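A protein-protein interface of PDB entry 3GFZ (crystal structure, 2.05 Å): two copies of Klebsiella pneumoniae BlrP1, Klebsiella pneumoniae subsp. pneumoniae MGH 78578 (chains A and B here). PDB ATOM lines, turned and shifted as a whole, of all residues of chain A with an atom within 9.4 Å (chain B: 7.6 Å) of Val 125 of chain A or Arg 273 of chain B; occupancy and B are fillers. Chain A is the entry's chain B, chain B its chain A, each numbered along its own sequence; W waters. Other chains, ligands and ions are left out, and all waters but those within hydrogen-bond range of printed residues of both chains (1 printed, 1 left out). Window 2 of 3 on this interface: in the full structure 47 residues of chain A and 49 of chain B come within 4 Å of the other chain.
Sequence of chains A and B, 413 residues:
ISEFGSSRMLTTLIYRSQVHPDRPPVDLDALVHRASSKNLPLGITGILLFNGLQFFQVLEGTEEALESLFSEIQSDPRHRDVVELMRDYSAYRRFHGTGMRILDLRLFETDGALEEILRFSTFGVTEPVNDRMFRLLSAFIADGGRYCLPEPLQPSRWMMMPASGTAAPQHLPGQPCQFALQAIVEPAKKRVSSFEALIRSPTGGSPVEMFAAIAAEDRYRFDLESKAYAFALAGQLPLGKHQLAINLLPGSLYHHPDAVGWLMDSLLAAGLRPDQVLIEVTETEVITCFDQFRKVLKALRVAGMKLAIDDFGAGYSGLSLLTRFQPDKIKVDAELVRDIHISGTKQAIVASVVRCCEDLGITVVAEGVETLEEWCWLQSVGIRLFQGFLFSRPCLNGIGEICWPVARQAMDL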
ATOM      1  N   ALA A  91     -12.658  -9.464   1.655  1.00  0.00           N
ATOM      2  CA  ALA A  91     -13.274  -9.580   0.338  1.00  0.00           C
ATOM      3  C   ALA A  91     -13.957  -8.287  -0.098  1.00  0.00           C
ATOM      4  O   ALA A  91     -14.196  -8.091  -1.284  1.00  0.00           O
ATOM      5  CB  ALA A  91     -14.267 -10.720   0.326  1.00  0.00           C
ATOM      6  N   TYR A  92     -14.279  -7.410   0.855  1.00  0.00           N
ATOM      7  CA  TYR A  92     -14.996  -6.188   0.543  1.00  0.00           C
ATOM      8  C   TYR A  92     -14.838  -5.162   1.663  1.00  0.00           C
ATOM      9  O   TYR A  92     -14.564  -5.505   2.809  1.00  0.00           O
ATOM     10  CB  TYR A  92     -16.481  -6.501   0.297  1.00  0.00           C
ATOM     11  CG  TYR A  92     -17.226  -6.970   1.536  1.00  0.00           C
ATOM     12  CD1 TYR A  92     -17.227  -8.312   1.918  1.00  0.00           C
ATOM     13  CD2 TYR A  92     -17.924  -6.069   2.325  1.00  0.00           C
ATOM     14  CE1 TYR A  92     -17.911  -8.733   3.063  1.00  0.00           C
ATOM     15  CE2 TYR A  92     -18.603  -6.472   3.457  1.00  0.00           C
ATOM     16  CZ  TYR A  92     -18.600  -7.802   3.825  1.00  0.00           C
ATOM     17  OH  TYR A  92     -19.286  -8.183   4.964  1.00  0.00           O
ATOM     18  N   THR A 122     -21.592  -1.249   5.467  1.00  0.00           N
ATOM     19  CA  THR A 122     -22.193  -2.423   4.841  1.00  0.00           C
ATOM     20  C   THR A 122     -21.497  -3.662   5.406  1.00  0.00           C
ATOM     21  O   THR A 122     -20.290  -3.792   5.260  1.00  0.00           O
ATOM     22  CB  THR A 122     -21.993  -2.404   3.292  1.00  0.00           C
ATOM     23  OG1 THR A 122     -20.593  -2.416   2.976  1.00  0.00           O
ATOM     24  CG2 THR A 122     -22.637  -1.160   2.658  1.00  0.00           C
ATOM     25  N   PHE A 123     -22.237  -4.550   6.071  1.00  0.00           N
ATOM     26  CA  PHE A 123     -21.665  -5.806   6.590  1.00  0.00           C
ATOM     27  C   PHE A 123     -22.191  -7.043   5.856  1.00  0.00           C
ATOM     28  O   PHE A 123     -22.434  -8.088   6.459  1.00  0.00           O
ATOM     29  CB  PHE A 123     -21.901  -5.907   8.100  1.00  0.00           C
ATOM     30  CG  PHE A 123     -21.237  -4.814   8.878  1.00  0.00           C
ATOM     31  CD1 PHE A 123     -19.884  -4.885   9.178  1.00  0.00           C
ATOM     32  CD2 PHE A 123     -21.951  -3.698   9.290  1.00  0.00           C
ATOM     33  CE1 PHE A 123     -19.258  -3.871   9.882  1.00  0.00           C
ATOM     34  CE2 PHE A 123     -21.328  -2.677   9.986  1.00  0.00           C
ATOM     35  CZ  PHE A 123     -19.984  -2.761  10.289  1.00  0.00           C
ATOM     36  N   GLY A 124     -22.339  -6.934   4.540  1.00  0.00           N
ATOM     37  CA  GLY A 124     -22.785  -8.054   3.720  1.00  0.00           C
ATOM     38  C   GLY A 124     -24.281  -8.275   3.810  1.00  0.00           C
ATOM     39  O   GLY A 124     -25.012  -7.397   4.270  1.00  0.00           O
ATOM     40  N   VAL A 125     -24.729  -9.451   3.374  1.00  0.00           N
ATOM     41  CA  VAL A 125     -26.164  -9.762   3.300  1.00  0.00           C
ATOM     42  C   VAL A 125     -26.734 -10.365   4.587  1.00  0.00           C
ATOM     43  O   VAL A 125     -27.954 -10.360   4.782  1.00  0.00           O
ATOM     44  CB  VAL A 125     -26.499 -10.721   2.132  1.00  0.00           C
ATOM     45  CG1 VAL A 125     -25.942 -10.182   0.819  1.00  0.00           C
ATOM     46  CG2 VAL A 125     -26.000 -12.148   2.401  1.00  0.00           C
ATOM     47  N   THR A 126     -25.864 -10.901   5.444  1.00  0.00           N
ATOM     48  CA  THR A 126     -26.299 -11.494   6.709  1.00  0.00           C
ATOM     49  C   THR A 126     -26.140 -10.462   7.815  1.00  0.00           C
ATOM     50  O   THR A 126     -25.428  -9.469   7.646  1.00  0.00           O
ATOM     51  CB  THR A 126     -25.516 -12.793   7.056  1.00  0.00           C
ATOM     52  OG1 THR A 126     -24.186 -12.473   7.489  1.00  0.00           O
ATOM     53  CG2 THR A 126     -25.455 -13.740   5.851  1.00  0.00           C
ATOM     54  N   GLU A 127     -26.805 -10.710   8.941  1.00  0.00           N
ATOM     55  CA  GLU A 127     -26.893  -9.739  10.038  1.00  0.00           C
ATOM     56  C   GLU A 127     -25.517  -9.191  10.406  1.00  0.00           C
ATOM     57  O   GLU A 127     -24.555  -9.955  10.447  1.00  0.00           O
ATOM     58  CB  GLU A 127     -27.529 -10.381  11.275  1.00  0.00           C
ATOM     59  CG  GLU A 127     -29.020 -10.674  11.135  1.00  0.00           C
ATOM     60  CD  GLU A 127     -29.899  -9.441  11.301  1.00  0.00           C
ATOM     61  OE1 GLU A 127     -29.610  -8.609  12.189  1.00  0.00           O
ATOM     62  OE2 GLU A 127     -30.890  -9.317  10.551  1.00  0.00           O
ATOM     63  N   PRO A 128     -25.417  -7.876  10.699  1.00  0.00           N
ATOM     64  CA  PRO A 128     -24.126  -7.252  11.033  1.00  0.00           C
ATOM     65  C   PRO A 128     -23.355  -8.002  12.111  1.00  0.00           C
ATOM     66  O   PRO A 128     -22.129  -8.038  12.093  1.00  0.00           O
ATOM     67  CB  PRO A 128     -24.527  -5.877  11.575  1.00  0.00           C
ATOM     68  CG  PRO A 128     -25.837  -5.599  11.007  1.00  0.00           C
ATOM     69  CD  PRO A 128     -26.523  -6.903  10.762  1.00  0.00           C
ATOM     70  N   VAL A 129     -24.089  -8.593  13.043  1.00  0.00           N
ATOM     71  CA  VAL A 129     -23.508  -9.354  14.139  1.00  0.00           C
ATOM     72  C   VAL A 129     -22.790 -10.637  13.695  1.00  0.00           C
ATOM     73  O   VAL A 129     -22.088 -11.239  14.490  1.00  0.00           O
ATOM     74  CB  VAL A 129     -24.585  -9.671  15.206  1.00  0.00           C
ATOM     75  CG1 VAL A 129     -25.559 -10.752  14.711  1.00  0.00           C
ATOM     76  CG2 VAL A 129     -23.945 -10.059  16.537  1.00  0.00           C
ATOM     77  N   ASN A 130     -22.958 -11.052  12.436  1.00  0.00           N
ATOM     78  CA  ASN A 130     -22.157 -12.141  11.870  1.00  0.00           C
ATOM     79  C   ASN A 130     -20.784 -11.689  11.365  1.00  0.00           C
ATOM     80  O   ASN A 130     -19.998 -12.518  10.906  1.00  0.00           O
ATOM     81  CB  ASN A 130     -22.924 -12.835  10.738  1.00  0.00           C
ATOM     82  CG  ASN A 130     -24.171 -13.553  11.234  1.00  0.00           C
ATOM     83  OD1 ASN A 130     -24.236 -13.985  12.381  1.00  0.00           O
ATOM     84  ND2 ASN A 130     -25.160 -13.693  10.363  1.00  0.00           N
ATOM     85  N   ASP A 131     -20.482 -10.393  11.476  1.00  0.00           N
ATOM     86  CA  ASP A 131     -19.213  -9.862  11.009  1.00  0.00           C
ATOM     87  C   ASP A 131     -18.313  -9.593  12.201  1.00  0.00           C
ATOM     88  O   ASP A 131     -18.690  -8.859  13.119  1.00  0.00           O
ATOM     89  CB  ASP A 131     -19.448  -8.584  10.204  1.00  0.00           C
ATOM     90  CG  ASP A 131     -18.292  -8.247   9.293  1.00  0.00           C
ATOM     91  OD1 ASP A 131     -17.165  -8.035   9.798  1.00  0.00           O
ATOM     92  OD2 ASP A 131     -18.512  -8.183   8.063  1.00  0.00           O
ATOM     93  N   LEU B 239     -32.609 -18.919   0.927  1.00  0.00           N
ATOM     94  CA  LEU B 239     -31.853 -18.748   2.175  1.00  0.00           C
ATOM     95  C   LEU B 239     -32.077 -17.363   2.786  1.00  0.00           C
ATOM     96  O   LEU B 239     -32.098 -17.223   4.009  1.00  0.00           O
ATOM     97  CB  LEU B 239     -30.357 -18.998   1.953  1.00  0.00           C
ATOM     98  CG  LEU B 239     -29.523 -19.179   3.226  1.00  0.00           C
ATOM     99  CD1 LEU B 239     -30.034 -20.319   4.104  1.00  0.00           C
ATOM    100  CD2 LEU B 239     -28.069 -19.411   2.865  1.00  0.00           C
ATOM    101  N   GLY B 240     -32.269 -16.352   1.938  1.00  0.00           N
ATOM    102  CA  GLY B 240     -32.550 -14.996   2.406  1.00  0.00           C
ATOM    103  C   GLY B 240     -31.297 -14.389   2.999  1.00  0.00           C
ATOM    104  O   GLY B 240     -30.219 -14.472   2.405  1.00  0.00           O
ATOM    105  N   LYS B 241     -31.425 -13.812   4.184  1.00  0.00           N
ATOM    106  CA  LYS B 241     -30.292 -13.191   4.854  1.00  0.00           C
ATOM    107  C   LYS B 241     -29.585 -14.143   5.830  1.00  0.00           C
ATOM    108  O   LYS B 241     -28.779 -13.694   6.628  1.00  0.00           O
ATOM    109  CB  LYS B 241     -30.752 -11.912   5.570  1.00  0.00           C
ATOM    110  CG  LYS B 241     -31.320 -10.854   4.610  1.00  0.00           C
ATOM    111  CD  LYS B 241     -31.816  -9.618   5.345  1.00  0.00           C
ATOM    112  CE  LYS B 241     -32.277  -8.543   4.368  1.00  0.00           C
ATOM    113  NZ  LYS B 241     -33.572  -8.868   3.705  1.00  0.00           N
ATOM    114  N   HIS B 242     -29.855 -15.449   5.755  1.00  0.00           N
ATOM    115  CA  HIS B 242     -29.289 -16.405   6.707  1.00  0.00           C
ATOM    116  C   HIS B 242     -27.986 -17.031   6.209  1.00  0.00           C
ATOM    117  O   HIS B 242     -27.748 -17.131   5.009  1.00  0.00           O
ATOM    118  CB  HIS B 242     -30.287 -17.526   7.000  1.00  0.00           C
ATOM    119  CG  HIS B 242     -31.586 -17.051   7.568  1.00  0.00           C
ATOM    120  ND1 HIS B 242     -32.774 -17.127   6.873  1.00  0.00           N
ATOM    121  CD2 HIS B 242     -31.886 -16.501   8.767  1.00  0.00           C
ATOM    122  CE1 HIS B 242     -33.750 -16.640   7.620  1.00  0.00           C
ATOM    123  NE2 HIS B 242     -33.238 -16.254   8.775  1.00  0.00           N
ATOM    124  N   GLN B 243     -27.154 -17.451   7.155  1.00  0.00           N
ATOM    125  CA  GLN B 243     -25.930 -18.192   6.855  1.00  0.00           C
ATOM    126  C   GLN B 243     -26.202 -19.665   6.594  1.00  0.00           C
ATOM    127  O   GLN B 243     -27.102 -20.241   7.190  1.00  0.00           O
ATOM    128  CB  GLN B 243     -24.950 -18.112   8.027  1.00  0.00           C
ATOM    129  CG  GLN B 243     -23.982 -16.949   7.988  1.00  0.00           C
ATOM    130  CD  GLN B 243     -22.800 -17.162   8.923  1.00  0.00           C
ATOM    131  OE1 GLN B 243     -22.366 -18.295   9.142  1.00  0.00           O
ATOM    132  NE2 GLN B 243     -22.280 -16.075   9.482  1.00  0.00           N
ATOM    133  N   LEU B 244     -25.398 -20.264   5.718  1.00  0.00           N
ATOM    134  CA  LEU B 244     -25.342 -21.718   5.538  1.00  0.00           C
ATOM    135  C   LEU B 244     -23.976 -22.256   5.998  1.00  0.00           C
ATOM    136  O   LEU B 244     -22.954 -21.854   5.448  1.00  0.00           O
ATOM    137  CB  LEU B 244     -25.570 -22.068   4.063  1.00  0.00           C
ATOM    138  CG  LEU B 244     -25.447 -23.546   3.681  1.00  0.00           C
ATOM    139  CD1 LEU B 244     -26.603 -24.348   4.238  1.00  0.00           C
ATOM    140  CD2 LEU B 244     -25.369 -23.692   2.177  1.00  0.00           C
ATOM    141  N   MET B 264     -16.582 -21.111  -4.725  1.00  0.00           N
ATOM    142  CA  MET B 264     -17.080 -19.805  -5.184  1.00  0.00           C
ATOM    143  C   MET B 264     -18.041 -19.943  -6.361  1.00  0.00           C
ATOM    144  O   MET B 264     -19.164 -19.467  -6.296  1.00  0.00           O
ATOM    145  CB  MET B 264     -15.929 -18.887  -5.617  1.00  0.00           C
ATOM    146  CG  MET B 264     -15.347 -17.989  -4.550  1.00  0.00           C
ATOM    147  SD  MET B 264     -16.508 -16.774  -3.893  1.00  0.00           S
ATOM    148  CE  MET B 264     -16.920 -17.533  -2.358  1.00  0.00           C
ATOM    149  N   LEU B 267     -21.452 -21.830  -5.375  1.00  0.00           N
ATOM    150  CA  LEU B 267     -22.384 -21.086  -4.526  1.00  0.00           C
ATOM    151  C   LEU B 267     -22.985 -19.906  -5.283  1.00  0.00           C
ATOM    152  O   LEU B 267     -24.175 -19.631  -5.141  1.00  0.00           O
ATOM    153  CB  LEU B 267     -21.738 -20.634  -3.206  1.00  0.00           C
ATOM    154  CG  LEU B 267     -20.629 -19.582  -3.154  1.00  0.00           C
ATOM    155  CD1 LEU B 267     -21.158 -18.150  -3.115  1.00  0.00           C
ATOM    156  CD2 LEU B 267     -19.750 -19.830  -1.943  1.00  0.00           C
ATOM    157  N   LEU B 268     -22.171 -19.230  -6.098  1.00  0.00           N
ATOM    158  CA  LEU B 268     -22.659 -18.106  -6.897  1.00  0.00           C
ATOM    159  C   LEU B 268     -23.678 -18.576  -7.931  1.00  0.00           C
ATOM    160  O   LEU B 268     -24.667 -17.890  -8.179  1.00  0.00           O
ATOM    161  CB  LEU B 268     -21.510 -17.356  -7.582  1.00  0.00           C
ATOM    162  CG  LEU B 268     -20.531 -16.561  -6.713  1.00  0.00           C
ATOM    163  CD1 LEU B 268     -19.332 -16.114  -7.551  1.00  0.00           C
ATOM    164  CD2 LEU B 268     -21.190 -15.364  -6.045  1.00  0.00           C
ATOM    165  N   ALA B 270     -25.643 -21.038  -7.544  1.00  0.00           N
ATOM    166  CA  ALA B 270     -26.837 -21.322  -6.767  1.00  0.00           C
ATOM    167  C   ALA B 270     -27.461 -20.049  -6.189  1.00  0.00           C
ATOM    168  O   ALA B 270     -28.404 -20.129  -5.410  1.00  0.00           O
ATOM    169  CB  ALA B 270     -26.507 -22.298  -5.656  1.00  0.00           C
ATOM    170  N   GLY B 271     -26.940 -18.883  -6.565  1.00  0.00           N
ATOM    171  CA  GLY B 271     -27.508 -17.603  -6.152  1.00  0.00           C
ATOM    172  C   GLY B 271     -27.186 -17.166  -4.735  1.00  0.00           C
ATOM    173  O   GLY B 271     -27.883 -16.313  -4.185  1.00  0.00           O
ATOM    174  N   LEU B 272     -26.135 -17.725  -4.139  1.00  0.00           N
ATOM    175  CA  LEU B 272     -25.714 -17.327  -2.792  1.00  0.00           C
ATOM    176  C   LEU B 272     -24.590 -16.311  -2.860  1.00  0.00           C
ATOM    177  O   LEU B 272     -24.023 -16.083  -3.917  1.00  0.00           O
ATOM    178  CB  LEU B 272     -25.244 -18.540  -1.989  1.00  0.00           C
ATOM    179  CG  LEU B 272     -26.233 -19.699  -1.877  1.00  0.00           C
ATOM    180  CD1 LEU B 272     -25.555 -20.894  -1.268  1.00  0.00           C
ATOM    181  CD2 LEU B 272     -27.449 -19.313  -1.066  1.00  0.00           C
ATOM    182  N   ARG B 273     -24.281 -15.708  -1.716  1.00  0.00           N
ATOM    183  CA  ARG B 273     -23.160 -14.785  -1.587  1.00  0.00           C
ATOM    184  C   ARG B 273     -22.049 -15.417  -0.745  1.00  0.00           C
ATOM    185  O   ARG B 273     -22.342 -16.180   0.174  1.00  0.00           O
ATOM    186  CB  ARG B 273     -23.626 -13.485  -0.935  1.00  0.00           C
ATOM    187  CG  ARG B 273     -24.622 -12.670  -1.773  1.00  0.00           C
ATOM    188  CD  ARG B 273     -24.036 -12.213  -3.100  1.00  0.00           C
ATOM    189  NE  ARG B 273     -22.806 -11.446  -2.904  1.00  0.00           N
ATOM    190  CZ  ARG B 273     -21.846 -11.274  -3.814  1.00  0.00           C
ATOM    191  NH1 ARG B 273     -21.929 -11.818  -5.028  1.00  0.00           N
ATOM    192  NH2 ARG B 273     -20.775 -10.549  -3.499  1.00  0.00           N
ATOM    193  N   PRO B 274     -20.771 -15.099  -1.050  1.00  0.00           N
ATOM    194  CA  PRO B 274     -19.639 -15.681  -0.312  1.00  0.00           C
ATOM    195  C   PRO B 274     -19.748 -15.535   1.207  1.00  0.00           C
ATOM    196  O   PRO B 274     -19.614 -16.520   1.932  1.00  0.00           O
ATOM    197  CB  PRO B 274     -18.443 -14.884  -0.840  1.00  0.00           C
ATOM    198  CG  PRO B 274     -18.845 -14.473  -2.196  1.00  0.00           C
ATOM    199  CD  PRO B 274     -20.301 -14.183  -2.105  1.00  0.00           C
ATOM    200  N   ASP B 275     -20.032 -14.316   1.669  1.00  0.00           N
ATOM    201  CA  ASP B 275     -20.195 -14.014   3.105  1.00  0.00           C
ATOM    202  C   ASP B 275     -21.373 -14.718   3.793  1.00  0.00           C
ATOM    203  O   ASP B 275     -21.505 -14.663   5.010  1.00  0.00           O
ATOM    204  CB  ASP B 275     -20.305 -12.497   3.313  1.00  0.00           C
ATOM    205  CG  ASP B 275     -21.410 -11.868   2.480  1.00  0.00           C
ATOM    206  OD1 ASP B 275     -21.127 -11.426   1.344  1.00  0.00           O
ATOM    207  OD2 ASP B 275     -22.562 -11.845   2.948  1.00  0.00           O
ATOM    208  N   GLN B 276     -22.222 -15.354   2.997  1.00  0.00           N
ATOM    209  CA  GLN B 276     -23.346 -16.160   3.456  1.00  0.00           C
ATOM    210  C   GLN B 276     -22.926 -17.590   3.772  1.00  0.00           C
ATOM    211  O   GLN B 276     -23.646 -18.319   4.447  1.00  0.00           O
ATOM    212  CB  GLN B 276     -24.367 -16.224   2.317  1.00  0.00           C
ATOM    213  CG  GLN B 276     -25.781 -16.456   2.722  1.00  0.00           C
ATOM    214  CD  GLN B 276     -26.745 -16.083   1.624  1.00  0.00           C
ATOM    215  OE1 GLN B 276     -26.416 -16.131   0.425  1.00  0.00           O
ATOM    216  NE2 GLN B 276     -27.941 -15.701   2.016  1.00  0.00           N
ATOM    217  N   VAL B 277     -21.787 -18.014   3.229  1.00  0.00           N
ATOM    218  CA  VAL B 277     -21.360 -19.387   3.365  1.00  0.00           C
ATOM    219  C   VAL B 277     -20.251 -19.455   4.391  1.00  0.00           C
ATOM    220  O   VAL B 277     -19.315 -18.644   4.385  1.00  0.00           O
ATOM    221  CB  VAL B 277     -20.916 -19.975   2.011  1.00  0.00           C
ATOM    222  CG1 VAL B 277     -20.372 -21.409   2.174  1.00  0.00           C
ATOM    223  CG2 VAL B 277     -22.095 -19.952   1.047  1.00  0.00           C
ATOM    224  N   LEU B 278     -20.371 -20.444   5.266  1.00  0.00           N
ATOM    225  CA  LEU B 278     -19.411 -20.673   6.311  1.00  0.00           C
ATOM    226  C   LEU B 278     -18.945 -22.123   6.257  1.00  0.00           C
ATOM    227  O   LEU B 278     -19.764 -23.046   6.178  1.00  0.00           O
ATOM    228  CB  LEU B 278     -20.053 -20.363   7.655  1.00  0.00           C
ATOM    229  CG  LEU B 278     -19.264 -20.750   8.900  1.00  0.00           C
ATOM    230  CD1 LEU B 278     -19.242 -19.607   9.903  1.00  0.00           C
ATOM    231  CD2 LEU B 278     -19.877 -21.995   9.498  1.00  0.00           C
ATOM    232  N   ALA B 303     -11.751 -14.609  -0.706  1.00  0.00           N
ATOM    233  CA  ALA B 303     -13.026 -14.877  -1.371  1.00  0.00           C
ATOM    234  C   ALA B 303     -14.233 -14.352  -0.585  1.00  0.00           C
ATOM    235  O   ALA B 303     -15.269 -14.056  -1.171  1.00  0.00           O
ATOM    236  CB  ALA B 303     -13.178 -16.360  -1.619  1.00  0.00           C
ATOM    237  N   GLY B 304     -14.107 -14.266   0.737  1.00  0.00           N
ATOM    238  CA  GLY B 304     -15.155 -13.714   1.589  1.00  0.00           C
ATOM    239  C   GLY B 304     -15.987 -14.732   2.346  1.00  0.00           C
ATOM    240  O   GLY B 304     -16.887 -14.354   3.094  1.00  0.00           O
ATOM    241  N   MET B 305     -15.698 -16.019   2.166  1.00  0.00           N
ATOM    242  CA  MET B 305     -16.382 -17.061   2.934  1.00  0.00           C
ATOM    243  C   MET B 305     -15.898 -17.043   4.378  1.00  0.00           C
ATOM    244  O   MET B 305     -14.777 -16.611   4.664  1.00  0.00           O
ATOM    245  CB  MET B 305     -16.162 -18.443   2.307  1.00  0.00           C
ATOM    246  CG  MET B 305     -16.901 -18.627   1.002  1.00  0.00           C
ATOM    247  SD  MET B 305     -16.490 -20.129   0.083  1.00  0.00           S
ATOM    248  CE  MET B 305     -14.854 -19.769  -0.496  1.00  0.00           C
HETATM  249  O   HOH W   1     -23.017 -11.228   5.401  1.00  0.00           O
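OE1 of Gln 276 of chain B sits at hydrogen-bond distance from N of Arg 273 of chain B (3.1 Å).
OG1 of Thr 126 of chain A is in hydrogen-bond range of ND2 of Asn 130 of chain A, 3.3 Å away.
The backbone NH (N) of Asp 275 of chain B lies close to the backbone carbonyl oxygen (O) of Gly 304 of chain B (3.5 Å).
OH of Tyr 92 of chain A sits at hydrogen-bond distance from N of Gly 124 of chain A (3.3 Å).
No position is printed for both chains.
Among the printed residues, no Asp or Glu carboxylate lies within 4 Å of a Lys or Arg side-chain nitrogen of the other chain.
Among the printed residues, pairs that only touch across the chains: Ala 91 of chain A with Ala 303 of chain B, Ala 91 of chain A with Gly 304 of chain B, Gly 124 of chain A with Asp 275 of chain B, Val 125 of chain A with Lys 241 of chain B, Val 125 of chain A with Arg 273 of chain B, Thr 126 of chain A with Lys 241 of chain B and Asn 130 of chain A with Gln 243 of chain B.
The backbone NH of Val 125 of chain A is in hydrogen-bond range of the side-chain carboxylate of Asp 275 of chain B, at 3.3 Å.
Of the printed residues of chain B, Ala 91 of chain A touches Ala 303 and Gly 304.
Val 125 of chain A touches just these residues of chain B: Lys 241, Arg 273 and Asp 275.
Printed residues of chain B within 4 Å of Thr 126 of chain A: Lys 241 (3.3 Å).
Of the printed residues of chain B, Asn 130 of chain A touches Gln 243 (3.5 Å).
Printed residues of chain A within 4 Å of Lys 241 of chain B: Val 125 and Thr 126.
Of the printed residues of chain A, Gln 243 of chain B touches Asn 130.
Ala 270 of chain B touches none of the printed residues of chain A.
Arg 273 of chain B touches just one residue of chain A: Val 125.
The nearest residue of chain A that does not touch Arg 273 of chain B is Tyr 92 of chain A (6.9 Å).
The nearest printed residue of chain A that does not touch Gln 243 of chain B is Thr 126 of chain A (4.1 Å).
Water W1 lies within hydrogen-bond range of the side-chain carboxylate of Asp 275 of chain B, the side-chain hydroxyl of Thr 126 of chain A, the backbone NH of Val 125 of chain A and the backbone carbonyl oxygen of Phe 123 of chain A.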
